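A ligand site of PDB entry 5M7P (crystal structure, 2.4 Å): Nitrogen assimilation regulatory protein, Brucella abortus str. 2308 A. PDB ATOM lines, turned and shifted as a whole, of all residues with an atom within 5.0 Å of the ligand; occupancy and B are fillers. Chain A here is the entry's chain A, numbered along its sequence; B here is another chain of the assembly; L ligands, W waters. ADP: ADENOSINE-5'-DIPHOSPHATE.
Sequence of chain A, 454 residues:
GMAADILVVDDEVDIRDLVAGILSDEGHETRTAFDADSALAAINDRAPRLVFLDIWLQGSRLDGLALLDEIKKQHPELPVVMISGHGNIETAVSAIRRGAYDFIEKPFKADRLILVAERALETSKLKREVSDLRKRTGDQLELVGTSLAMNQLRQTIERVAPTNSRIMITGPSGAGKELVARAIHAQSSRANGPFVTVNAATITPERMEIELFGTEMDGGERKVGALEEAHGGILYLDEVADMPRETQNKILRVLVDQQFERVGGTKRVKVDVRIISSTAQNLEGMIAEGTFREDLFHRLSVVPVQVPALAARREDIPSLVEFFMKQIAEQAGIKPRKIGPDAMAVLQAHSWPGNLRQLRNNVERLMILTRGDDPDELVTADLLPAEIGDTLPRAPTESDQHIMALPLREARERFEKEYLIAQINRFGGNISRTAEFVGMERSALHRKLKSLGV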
ATOM      1  N   LEU A 143     -15.004  -6.782 -20.861  1.00  0.00           N
ATOM      2  CA  LEU A 143     -15.709  -7.351 -22.023  1.00  0.00           C
ATOM      3  C   LEU A 143     -15.650  -6.455 -23.245  1.00  0.00           C
ATOM      4  O   LEU A 143     -16.362  -5.453 -23.338  1.00  0.00           O
ATOM      5  CB  LEU A 143     -17.165  -7.699 -21.686  1.00  0.00           C
ATOM      6  CG  LEU A 143     -17.381  -8.897 -20.762  1.00  0.00           C
ATOM      7  CD1 LEU A 143     -18.800  -8.975 -20.346  1.00  0.00           C
ATOM      8  CD2 LEU A 143     -17.085 -10.178 -21.481  1.00  0.00           C
ATOM      9  N   VAL A 144     -14.767  -6.811 -24.179  1.00  0.00           N
ATOM     10  CA  VAL A 144     -14.502  -6.045 -25.390  1.00  0.00           C
ATOM     11  C   VAL A 144     -15.609  -6.254 -26.434  1.00  0.00           C
ATOM     12  O   VAL A 144     -16.110  -7.366 -26.603  1.00  0.00           O
ATOM     13  CB  VAL A 144     -13.072  -6.370 -25.933  1.00  0.00           C
ATOM     14  CG1 VAL A 144     -12.784  -5.677 -27.271  1.00  0.00           C
ATOM     15  CG2 VAL A 144     -12.003  -6.031 -24.914  1.00  0.00           C
ATOM     16  N   MET A 150     -22.866  -7.230 -27.768  1.00  0.00           N
ATOM     17  CA  MET A 150     -22.019  -7.018 -26.592  1.00  0.00           C
ATOM     18  C   MET A 150     -22.609  -6.001 -25.633  1.00  0.00           C
ATOM     19  O   MET A 150     -22.517  -6.193 -24.412  1.00  0.00           O
ATOM     20  CB  MET A 150     -20.590  -6.593 -26.982  1.00  0.00           C
ATOM     21  CG  MET A 150     -19.665  -7.776 -27.245  1.00  0.00           C
ATOM     22  SD  MET A 150     -19.928  -9.263 -26.222  1.00  0.00           S
ATOM     23  CE  MET A 150     -19.264  -8.688 -24.638  1.00  0.00           C
ATOM     24  N   PRO A 172     -21.934 -21.008 -27.372  1.00  0.00           N
ATOM     25  CA  PRO A 172     -20.921 -21.968 -27.814  1.00  0.00           C
ATOM     26  C   PRO A 172     -19.593 -21.879 -27.050  1.00  0.00           C
ATOM     27  O   PRO A 172     -19.310 -20.868 -26.419  1.00  0.00           O
ATOM     28  CB  PRO A 172     -20.761 -21.645 -29.312  1.00  0.00           C
ATOM     29  CG  PRO A 172     -21.121 -20.219 -29.411  1.00  0.00           C
ATOM     30  CD  PRO A 172     -22.195 -19.975 -28.406  1.00  0.00           C
ATOM     31  N   SER A 173     -18.787 -22.953 -27.123  1.00  0.00           N
ATOM     32  CA  SER A 173     -17.466 -23.060 -26.498  1.00  0.00           C
ATOM     33  C   SER A 173     -16.523 -21.906 -26.903  1.00  0.00           C
ATOM     34  O   SER A 173     -16.402 -21.564 -28.103  1.00  0.00           O
ATOM     35  CB  SER A 173     -16.838 -24.399 -26.872  1.00  0.00           C
ATOM     36  OG  SER A 173     -17.635 -25.452 -26.335  1.00  0.00           O
ATOM     37  N   GLY A 174     -15.919 -21.271 -25.893  1.00  0.00           N
ATOM     38  CA  GLY A 174     -14.991 -20.160 -26.094  1.00  0.00           C
ATOM     39  C   GLY A 174     -15.630 -18.813 -26.356  1.00  0.00           C
ATOM     40  O   GLY A 174     -14.897 -17.843 -26.581  1.00  0.00           O
ATOM     41  N   ALA A 175     -16.970 -18.724 -26.296  1.00  0.00           N
ATOM     42  CA  ALA A 175     -17.700 -17.472 -26.516  1.00  0.00           C
ATOM     43  C   ALA A 175     -17.599 -16.446 -25.353  1.00  0.00           C
ATOM     44  O   ALA A 175     -17.785 -15.255 -25.585  1.00  0.00           O
ATOM     45  CB  ALA A 175     -19.167 -17.759 -26.846  1.00  0.00           C
ATOM     46  N   GLY A 176     -17.297 -16.913 -24.139  1.00  0.00           N
ATOM     47  CA  GLY A 176     -17.111 -16.051 -22.972  1.00  0.00           C
ATOM     48  C   GLY A 176     -18.056 -16.277 -21.808  1.00  0.00           C
ATOM     49  O   GLY A 176     -18.231 -15.375 -21.009  1.00  0.00           O
ATOM     50  N   LYS A 177     -18.639 -17.493 -21.696  1.00  0.00           N
ATOM     51  CA  LYS A 177     -19.586 -17.870 -20.643  1.00  0.00           C
ATOM     52  C   LYS A 177     -19.002 -17.756 -19.266  1.00  0.00           C
ATOM     53  O   LYS A 177     -19.644 -17.164 -18.402  1.00  0.00           O
ATOM     54  CB  LYS A 177     -20.139 -19.284 -20.876  1.00  0.00           C
ATOM     55  CG  LYS A 177     -20.981 -19.455 -22.147  1.00  0.00           C
ATOM     56  CD  LYS A 177     -21.676 -20.832 -22.145  1.00  0.00           C
ATOM     57  CE  LYS A 177     -20.730 -22.010 -22.245  1.00  0.00           C
ATOM     58  NZ  LYS A 177     -19.842 -21.932 -23.449  1.00  0.00           N
ATOM     59  N   GLU A 178     -17.780 -18.299 -19.046  1.00  0.00           N
ATOM     60  CA  GLU A 178     -17.105 -18.217 -17.755  1.00  0.00           C
ATOM     61  C   GLU A 178     -16.773 -16.758 -17.423  1.00  0.00           C
ATOM     62  O   GLU A 178     -16.921 -16.361 -16.274  1.00  0.00           O
ATOM     63  CB  GLU A 178     -15.828 -19.058 -17.736  1.00  0.00           C
ATOM     64  CG  GLU A 178     -15.185 -19.057 -16.362  1.00  0.00           C
ATOM     65  CD  GLU A 178     -14.146 -20.103 -16.070  1.00  0.00           C
ATOM     66  OE1 GLU A 178     -14.219 -21.214 -16.658  1.00  0.00           O
ATOM     67  OE2 GLU A 178     -13.278 -19.841 -15.215  1.00  0.00           O
ATOM     68  N   LEU A 179     -16.325 -15.977 -18.435  1.00  0.00           N
ATOM     69  CA  LEU A 179     -16.014 -14.563 -18.266  1.00  0.00           C
ATOM     70  C   LEU A 179     -17.277 -13.759 -17.868  1.00  0.00           C
ATOM     71  O   LEU A 179     -17.189 -12.893 -17.001  1.00  0.00           O
ATOM     72  CB  LEU A 179     -15.317 -14.002 -19.508  1.00  0.00           C
ATOM     73  CG  LEU A 179     -14.834 -12.554 -19.359  1.00  0.00           C
ATOM     74  CD1 LEU A 179     -13.767 -12.417 -18.247  1.00  0.00           C
ATOM     75  CD2 LEU A 179     -14.297 -12.053 -20.644  1.00  0.00           C
ATOM     76  N   TYR A 236     -19.963 -22.003  -9.927  1.00  0.00           N
ATOM     77  CA  TYR A 236     -20.051 -21.979 -11.380  1.00  0.00           C
ATOM     78  C   TYR A 236     -19.947 -23.407 -11.907  1.00  0.00           C
ATOM     79  O   TYR A 236     -18.901 -24.058 -11.806  1.00  0.00           O
ATOM     80  CB  TYR A 236     -18.994 -21.069 -12.010  1.00  0.00           C
ATOM     81  CG  TYR A 236     -19.095 -21.017 -13.517  1.00  0.00           C
ATOM     82  CD1 TYR A 236     -20.289 -20.672 -14.147  1.00  0.00           C
ATOM     83  CD2 TYR A 236     -18.005 -21.369 -14.325  1.00  0.00           C
ATOM     84  CE1 TYR A 236     -20.382 -20.635 -15.536  1.00  0.00           C
ATOM     85  CE2 TYR A 236     -18.097 -21.356 -15.718  1.00  0.00           C
ATOM     86  CZ  TYR A 236     -19.288 -20.982 -16.317  1.00  0.00           C
ATOM     87  OH  TYR A 236     -19.403 -20.954 -17.673  1.00  0.00           O
ATOM     88  N   ARG A 313     -21.193 -11.762 -34.130  1.00  0.00           N
ATOM     89  CA  ARG A 313     -20.681 -10.453 -33.693  1.00  0.00           C
ATOM     90  C   ARG A 313     -19.313 -10.170 -34.340  1.00  0.00           C
ATOM     91  O   ARG A 313     -18.385  -9.687 -33.690  1.00  0.00           O
ATOM     92  CB  ARG A 313     -20.646 -10.335 -32.143  1.00  0.00           C
ATOM     93  CG  ARG A 313     -20.009 -11.533 -31.466  1.00  0.00           C
ATOM     94  CD  ARG A 313     -19.506 -11.236 -30.082  1.00  0.00           C
ATOM     95  NE  ARG A 313     -19.577 -12.459 -29.293  1.00  0.00           N
ATOM     96  CZ  ARG A 313     -18.963 -12.666 -28.133  1.00  0.00           C
ATOM     97  NH1 ARG A 313     -18.157 -11.739 -27.623  1.00  0.00           N
ATOM     98  NH2 ARG A 313     -19.136 -13.812 -27.475  1.00  0.00           N
ATOM     99  N   LEU A 320     -11.160  -7.193 -31.044  1.00  0.00           N
ATOM    100  CA  LEU A 320     -10.743  -8.346 -30.269  1.00  0.00           C
ATOM    101  C   LEU A 320      -9.331  -8.705 -30.652  1.00  0.00           C
ATOM    102  O   LEU A 320      -8.533  -9.004 -29.773  1.00  0.00           O
ATOM    103  CB  LEU A 320     -11.707  -9.544 -30.395  1.00  0.00           C
ATOM    104  CG  LEU A 320     -13.081  -9.349 -29.692  1.00  0.00           C
ATOM    105  CD1 LEU A 320     -14.156 -10.251 -30.275  1.00  0.00           C
ATOM    106  CD2 LEU A 320     -12.979  -9.478 -28.158  1.00  0.00           C
ATOM    107  N   PHE A 323      -7.153  -6.171 -28.914  1.00  0.00           N
ATOM    108  CA  PHE A 323      -7.156  -6.450 -27.486  1.00  0.00           C
ATOM    109  C   PHE A 323      -6.259  -7.651 -27.165  1.00  0.00           C
ATOM    110  O   PHE A 323      -5.481  -7.597 -26.213  1.00  0.00           O
ATOM    111  CB  PHE A 323      -8.592  -6.656 -26.974  1.00  0.00           C
ATOM    112  CG  PHE A 323      -8.651  -7.158 -25.545  1.00  0.00           C
ATOM    113  CD1 PHE A 323      -8.417  -6.298 -24.485  1.00  0.00           C
ATOM    114  CD2 PHE A 323      -8.905  -8.503 -25.276  1.00  0.00           C
ATOM    115  CE1 PHE A 323      -8.422  -6.775 -23.174  1.00  0.00           C
ATOM    116  CE2 PHE A 323      -8.917  -8.968 -23.967  1.00  0.00           C
ATOM    117  CZ  PHE A 323      -8.684  -8.110 -22.921  1.00  0.00           C
ATOM    118  N   PHE A 324      -6.357  -8.732 -27.958  1.00  0.00           N
ATOM    119  CA  PHE A 324      -5.574  -9.943 -27.765  1.00  0.00           C
ATOM    120  C   PHE A 324      -4.094  -9.705 -28.043  1.00  0.00           C
ATOM    121  O   PHE A 324      -3.251 -10.211 -27.299  1.00  0.00           O
ATOM    122  CB  PHE A 324      -6.163 -11.123 -28.576  1.00  0.00           C
ATOM    123  CG  PHE A 324      -7.520 -11.616 -28.126  1.00  0.00           C
ATOM    124  CD1 PHE A 324      -7.820 -11.747 -26.766  1.00  0.00           C
ATOM    125  CD2 PHE A 324      -8.450 -12.072 -29.048  1.00  0.00           C
ATOM    126  CE1 PHE A 324      -9.060 -12.238 -26.352  1.00  0.00           C
ATOM    127  CE2 PHE A 324      -9.702 -12.559 -28.626  1.00  0.00           C
ATOM    128  CZ  PHE A 324     -10.000 -12.635 -27.283  1.00  0.00           C
ATOM    129  N   LEU A 356     -13.975 -17.051 -29.299  1.00  0.00           N
ATOM    130  CA  LEU A 356     -12.957 -16.115 -28.794  1.00  0.00           C
ATOM    131  C   LEU A 356     -11.689 -16.825 -28.327  1.00  0.00           C
ATOM    132  O   LEU A 356     -10.618 -16.321 -28.586  1.00  0.00           O
ATOM    133  CB  LEU A 356     -13.526 -15.164 -27.733  1.00  0.00           C
ATOM    134  CG  LEU A 356     -14.295 -13.988 -28.325  1.00  0.00           C
ATOM    135  CD1 LEU A 356     -15.781 -14.340 -28.634  1.00  0.00           C
ATOM    136  CD2 LEU A 356     -14.221 -12.793 -27.419  1.00  0.00           C
ATOM    137  N   ARG A 357     -11.798 -18.044 -27.766  1.00  0.00           N
ATOM    138  CA  ARG A 357     -10.588 -18.797 -27.415  1.00  0.00           C
ATOM    139  C   ARG A 357      -9.777 -19.092 -28.705  1.00  0.00           C
ATOM    140  O   ARG A 357      -8.572 -18.848 -28.747  1.00  0.00           O
ATOM    141  CB  ARG A 357     -10.920 -20.119 -26.693  1.00  0.00           C
ATOM    142  CG  ARG A 357      -9.643 -20.757 -26.117  1.00  0.00           C
ATOM    143  CD  ARG A 357      -9.832 -21.997 -25.275  1.00  0.00           C
ATOM    144  NE  ARG A 357     -11.220 -22.176 -24.903  1.00  0.00           N
ATOM    145  CZ  ARG A 357     -11.806 -21.615 -23.852  1.00  0.00           C
ATOM    146  NH1 ARG A 357     -11.096 -20.859 -23.020  1.00  0.00           N
ATOM    147  NH2 ARG A 357     -13.086 -21.800 -23.637  1.00  0.00           N
ATOM    148  N   ARG A 360      -8.154 -15.889 -30.085  1.00  0.00           N
ATOM    149  CA  ARG A 360      -7.001 -15.514 -29.233  1.00  0.00           C
ATOM    150  C   ARG A 360      -5.793 -16.394 -29.532  1.00  0.00           C
ATOM    151  O   ARG A 360      -4.690 -15.872 -29.704  1.00  0.00           O
ATOM    152  CB  ARG A 360      -7.378 -15.601 -27.750  1.00  0.00           C
ATOM    153  CG  ARG A 360      -6.298 -15.017 -26.838  1.00  0.00           C
ATOM    154  CD  ARG A 360      -6.382 -15.628 -25.467  1.00  0.00           C
ATOM    155  NE  ARG A 360      -5.463 -14.992 -24.538  1.00  0.00           N
ATOM    156  CZ  ARG A 360      -4.208 -15.381 -24.326  1.00  0.00           C
ATOM    157  NH1 ARG A 360      -3.691 -16.408 -25.001  1.00  0.00           N
ATOM    158  NH2 ARG A 360      -3.458 -14.743 -23.435  1.00  0.00           N
ATOM    159  N   GLN B 331      -8.439 -24.080 -17.826  1.00  0.00           N
ATOM    160  CA  GLN B 331      -8.893 -22.821 -18.406  1.00  0.00           C
ATOM    161  C   GLN B 331     -10.146 -22.934 -19.254  1.00  0.00           C
ATOM    162  O   GLN B 331     -11.028 -22.076 -19.149  1.00  0.00           O
ATOM    163  CB  GLN B 331      -7.776 -22.236 -19.283  1.00  0.00           C
ATOM    164  CG  GLN B 331      -6.698 -21.468 -18.526  1.00  0.00           C
ATOM    165  CD  GLN B 331      -5.383 -21.369 -19.280  1.00  0.00           C
ATOM    166  OE1 GLN B 331      -4.319 -21.367 -18.679  1.00  0.00           O
ATOM    167  NE2 GLN B 331      -5.418 -21.286 -20.605  1.00  0.00           N
ATOM    168  N   ALA B 332     -10.205 -23.947 -20.128  1.00  0.00           N
ATOM    169  CA  ALA B 332     -11.242 -24.122 -21.136  1.00  0.00           C
ATOM    170  C   ALA B 332     -12.329 -25.143 -20.866  1.00  0.00           C
ATOM    171  O   ALA B 332     -13.387 -25.079 -21.493  1.00  0.00           O
ATOM    172  CB  ALA B 332     -10.584 -24.463 -22.450  1.00  0.00           C
ATOM    173  N   ARG B 371     -11.991 -30.662 -29.426  1.00  0.00           N
ATOM    174  CA  ARG B 371     -12.949 -30.476 -28.338  1.00  0.00           C
ATOM    175  C   ARG B 371     -14.225 -31.343 -28.484  1.00  0.00           C
ATOM    176  O   ARG B 371     -14.653 -31.956 -27.504  1.00  0.00           O
ATOM    177  CB  ARG B 371     -13.294 -28.975 -28.185  1.00  0.00           C
ATOM    178  CG  ARG B 371     -14.574 -28.663 -27.391  1.00  0.00           C
ATOM    179  CD  ARG B 371     -14.547 -27.304 -26.745  1.00  0.00           C
ATOM    180  NE  ARG B 371     -14.857 -27.394 -25.327  1.00  0.00           N
ATOM    181  CZ  ARG B 371     -14.739 -26.406 -24.448  1.00  0.00           C
ATOM    182  NH1 ARG B 371     -14.277 -25.219 -24.830  1.00  0.00           N
ATOM    183  NH2 ARG B 371     -15.035 -26.601 -23.173  1.00  0.00           N
HETATM  184  PB  ADP L   1     -16.436 -20.209 -22.450  1.00  0.00           P
HETATM  185  O1B ADP L   1     -16.634 -20.274 -20.985  1.00  0.00           O
HETATM  186  O2B ADP L   1     -17.673 -19.930 -23.180  1.00  0.00           O
HETATM  187  O3B ADP L   1     -15.766 -21.479 -23.000  1.00  0.00           O
HETATM  188  PA  ADP L   1     -14.428 -18.216 -21.820  1.00  0.00           P
HETATM  189  O1A ADP L   1     -13.428 -19.165 -21.258  1.00  0.00           O
HETATM  190  O2A ADP L   1     -15.129 -17.473 -20.757  1.00  0.00           O
HETATM  191  O3A ADP L   1     -15.474 -18.976 -22.734  1.00  0.00           O
HETATM  192  O5' ADP L   1     -13.718 -17.274 -22.883  1.00  0.00           O
HETATM  193  C5' ADP L   1     -12.758 -17.691 -23.874  1.00  0.00           C
HETATM  194  C4' ADP L   1     -11.648 -16.677 -23.936  1.00  0.00           C
HETATM  195  O4' ADP L   1     -12.137 -15.435 -24.509  1.00  0.00           O
HETATM  196  C3' ADP L   1     -11.012 -16.280 -22.600  1.00  0.00           C
HETATM  197  O3' ADP L   1      -9.618 -16.048 -22.808  1.00  0.00           O
HETATM  198  C2' ADP L   1     -11.770 -15.004 -22.236  1.00  0.00           C
HETATM  199  O2' ADP L   1     -11.096 -14.133 -21.346  1.00  0.00           O
HETATM  200  C1' ADP L   1     -11.944 -14.365 -23.617  1.00  0.00           C
HETATM  201  N9  ADP L   1     -13.097 -13.465 -23.719  1.00  0.00           N
HETATM  202  C8  ADP L   1     -14.416 -13.841 -23.726  1.00  0.00           C
HETATM  203  N7  ADP L   1     -15.232 -12.854 -23.970  1.00  0.00           N
HETATM  204  C5  ADP L   1     -14.416 -11.751 -24.128  1.00  0.00           C
HETATM  205  C6  ADP L   1     -14.672 -10.402 -24.414  1.00  0.00           C
HETATM  206  N6  ADP L   1     -15.874  -9.938 -24.789  1.00  0.00           N
HETATM  207  N1  ADP L   1     -13.627  -9.536 -24.392  1.00  0.00           N
HETATM  208  C2  ADP L   1     -12.400 -10.018 -24.162  1.00  0.00           C
HETATM  209  N3  ADP L   1     -12.032 -11.282 -23.947  1.00  0.00           N
HETATM  210  C4  ADP L   1     -13.078 -12.114 -23.945  1.00  0.00           C
HETATM  211  O   HOH W   1     -17.746 -22.006 -19.536  1.00  0.00           O
HETATM  212  O   HOH W   2     -17.838 -12.600 -24.949  1.00  0.00           O
HETATM  213  O   HOH W   3     -14.459 -21.590 -19.823  1.00  0.00           O
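Water W1 lies within hydrogen-bond range of O1B of the ligand and OH of Tyr 236.
Water W3 lies within hydrogen-bond range of an oxygen (O1B) of the ligand (2.8 Å) and the side-chain carboxylate (OE1) of Glu 178 (3.2 Å).
Water W2 lies within hydrogen-bond range of the backbone carbonyl oxygen (O) of Ala 175 (2.7 Å), a nitrogen (N7) of the ligand (2.8 Å) and the guanidinium group (NH1) of Arg 313 (2.8 Å).
Leu 143 touches the ligand.
Met 150 touches the ligand.
Pro 172 touches the ligand (O to O2B, 3.7 Å).
Ser 173 touches the ligand (C to O3B, 3.999 Å).
Leu 320 touches the ligand (CD2 to N1, 3.8 Å).
Phe 323 touches the ligand (CE2 to C2, 3.6 Å).
CE1 of Phe 324 touches N3 of the ligand, at 3.9 Å.
CD2 of Leu 356 touches C5 of the ligand (3.5 Å).
Hydrophobic or aromatic side chains that line the ligand: Leu 143, Val 144, Met 150, Leu 179, Leu 320, Phe 323, Phe 324 and Leu 356.
16 residues have an atom within 4 Å of the ligand: Leu 143, Val 144, Met 150, Pro 172, Ser 173, Gly 174, Ala 175, Gly 176, Lys 177, Glu 178, Leu 179, Leu 320, Phe 323, Phe 324, Leu 356 and Arg 357.
The nearest printed residue that does not touch the ligand is Arg 313 (4.1 Å).
The side-chain amino group of Lys 177 is in hydrogen-bond range of the backbone carbonyl oxygen of Pro 172 (3.2 Å).
OH of Tyr 236 sits at hydrogen-bond distance from N of Glu 178 (3.4 Å).
The backbone carbonyl oxygen of Gly 174 lies within hydrogen-bond range of the backbone NH of Leu 356.
The guanidinium group (NH1) of Arg 313 sits at hydrogen-bond distance from the side-chain sulfur (SD) of Met 150 (3.4 Å).
The backbone carbonyl oxygen of Ala 175 sits at hydrogen-bond distance from the guanidinium group of Arg 313, at 2.7 Å.
N of Arg 357 lies within hydrogen-bond range of O of Gly 174, at 3.3 Å.
N of Glu 178 sits at hydrogen-bond distance from O1B of the ligand (3.0 Å).
A nitrogen (N6) of the ligand is in hydrogen-bond range of the backbone carbonyl oxygen (O) of Val 144.
The backbone NH (N) of Val 144 sits at hydrogen-bond distance from a nitrogen (N1) of the ligand (3.0 Å).
An oxygen (O3A) of the ligand lies within hydrogen-bond range of the backbone NH (N) of Gly 176 (3.1 Å).
The backbone NH (N) of Leu 179 sits at hydrogen-bond distance from an oxygen (O2A) of the ligand, at 3.0 Å.
The backbone NH of Gly 174 lies within hydrogen-bond range of an oxygen (O3B) of the ligand (2.9 Å).
An oxygen (O2B) of the ligand sits at hydrogen-bond distance from the backbone NH of Ala 175 (3.4 Å).
The backbone NH (N) of Lys 177 lies within hydrogen-bond range of an oxygen (O2B) of the ligand (3.0 Å).
The guanidinium group (NH2) of Arg 357 is in salt-bridge range of an oxygen (O3B) of the ligand (2.8 Å).
O2B of the ligand lies within salt-bridge range of NZ of Lys 177, 3.0 Å away.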
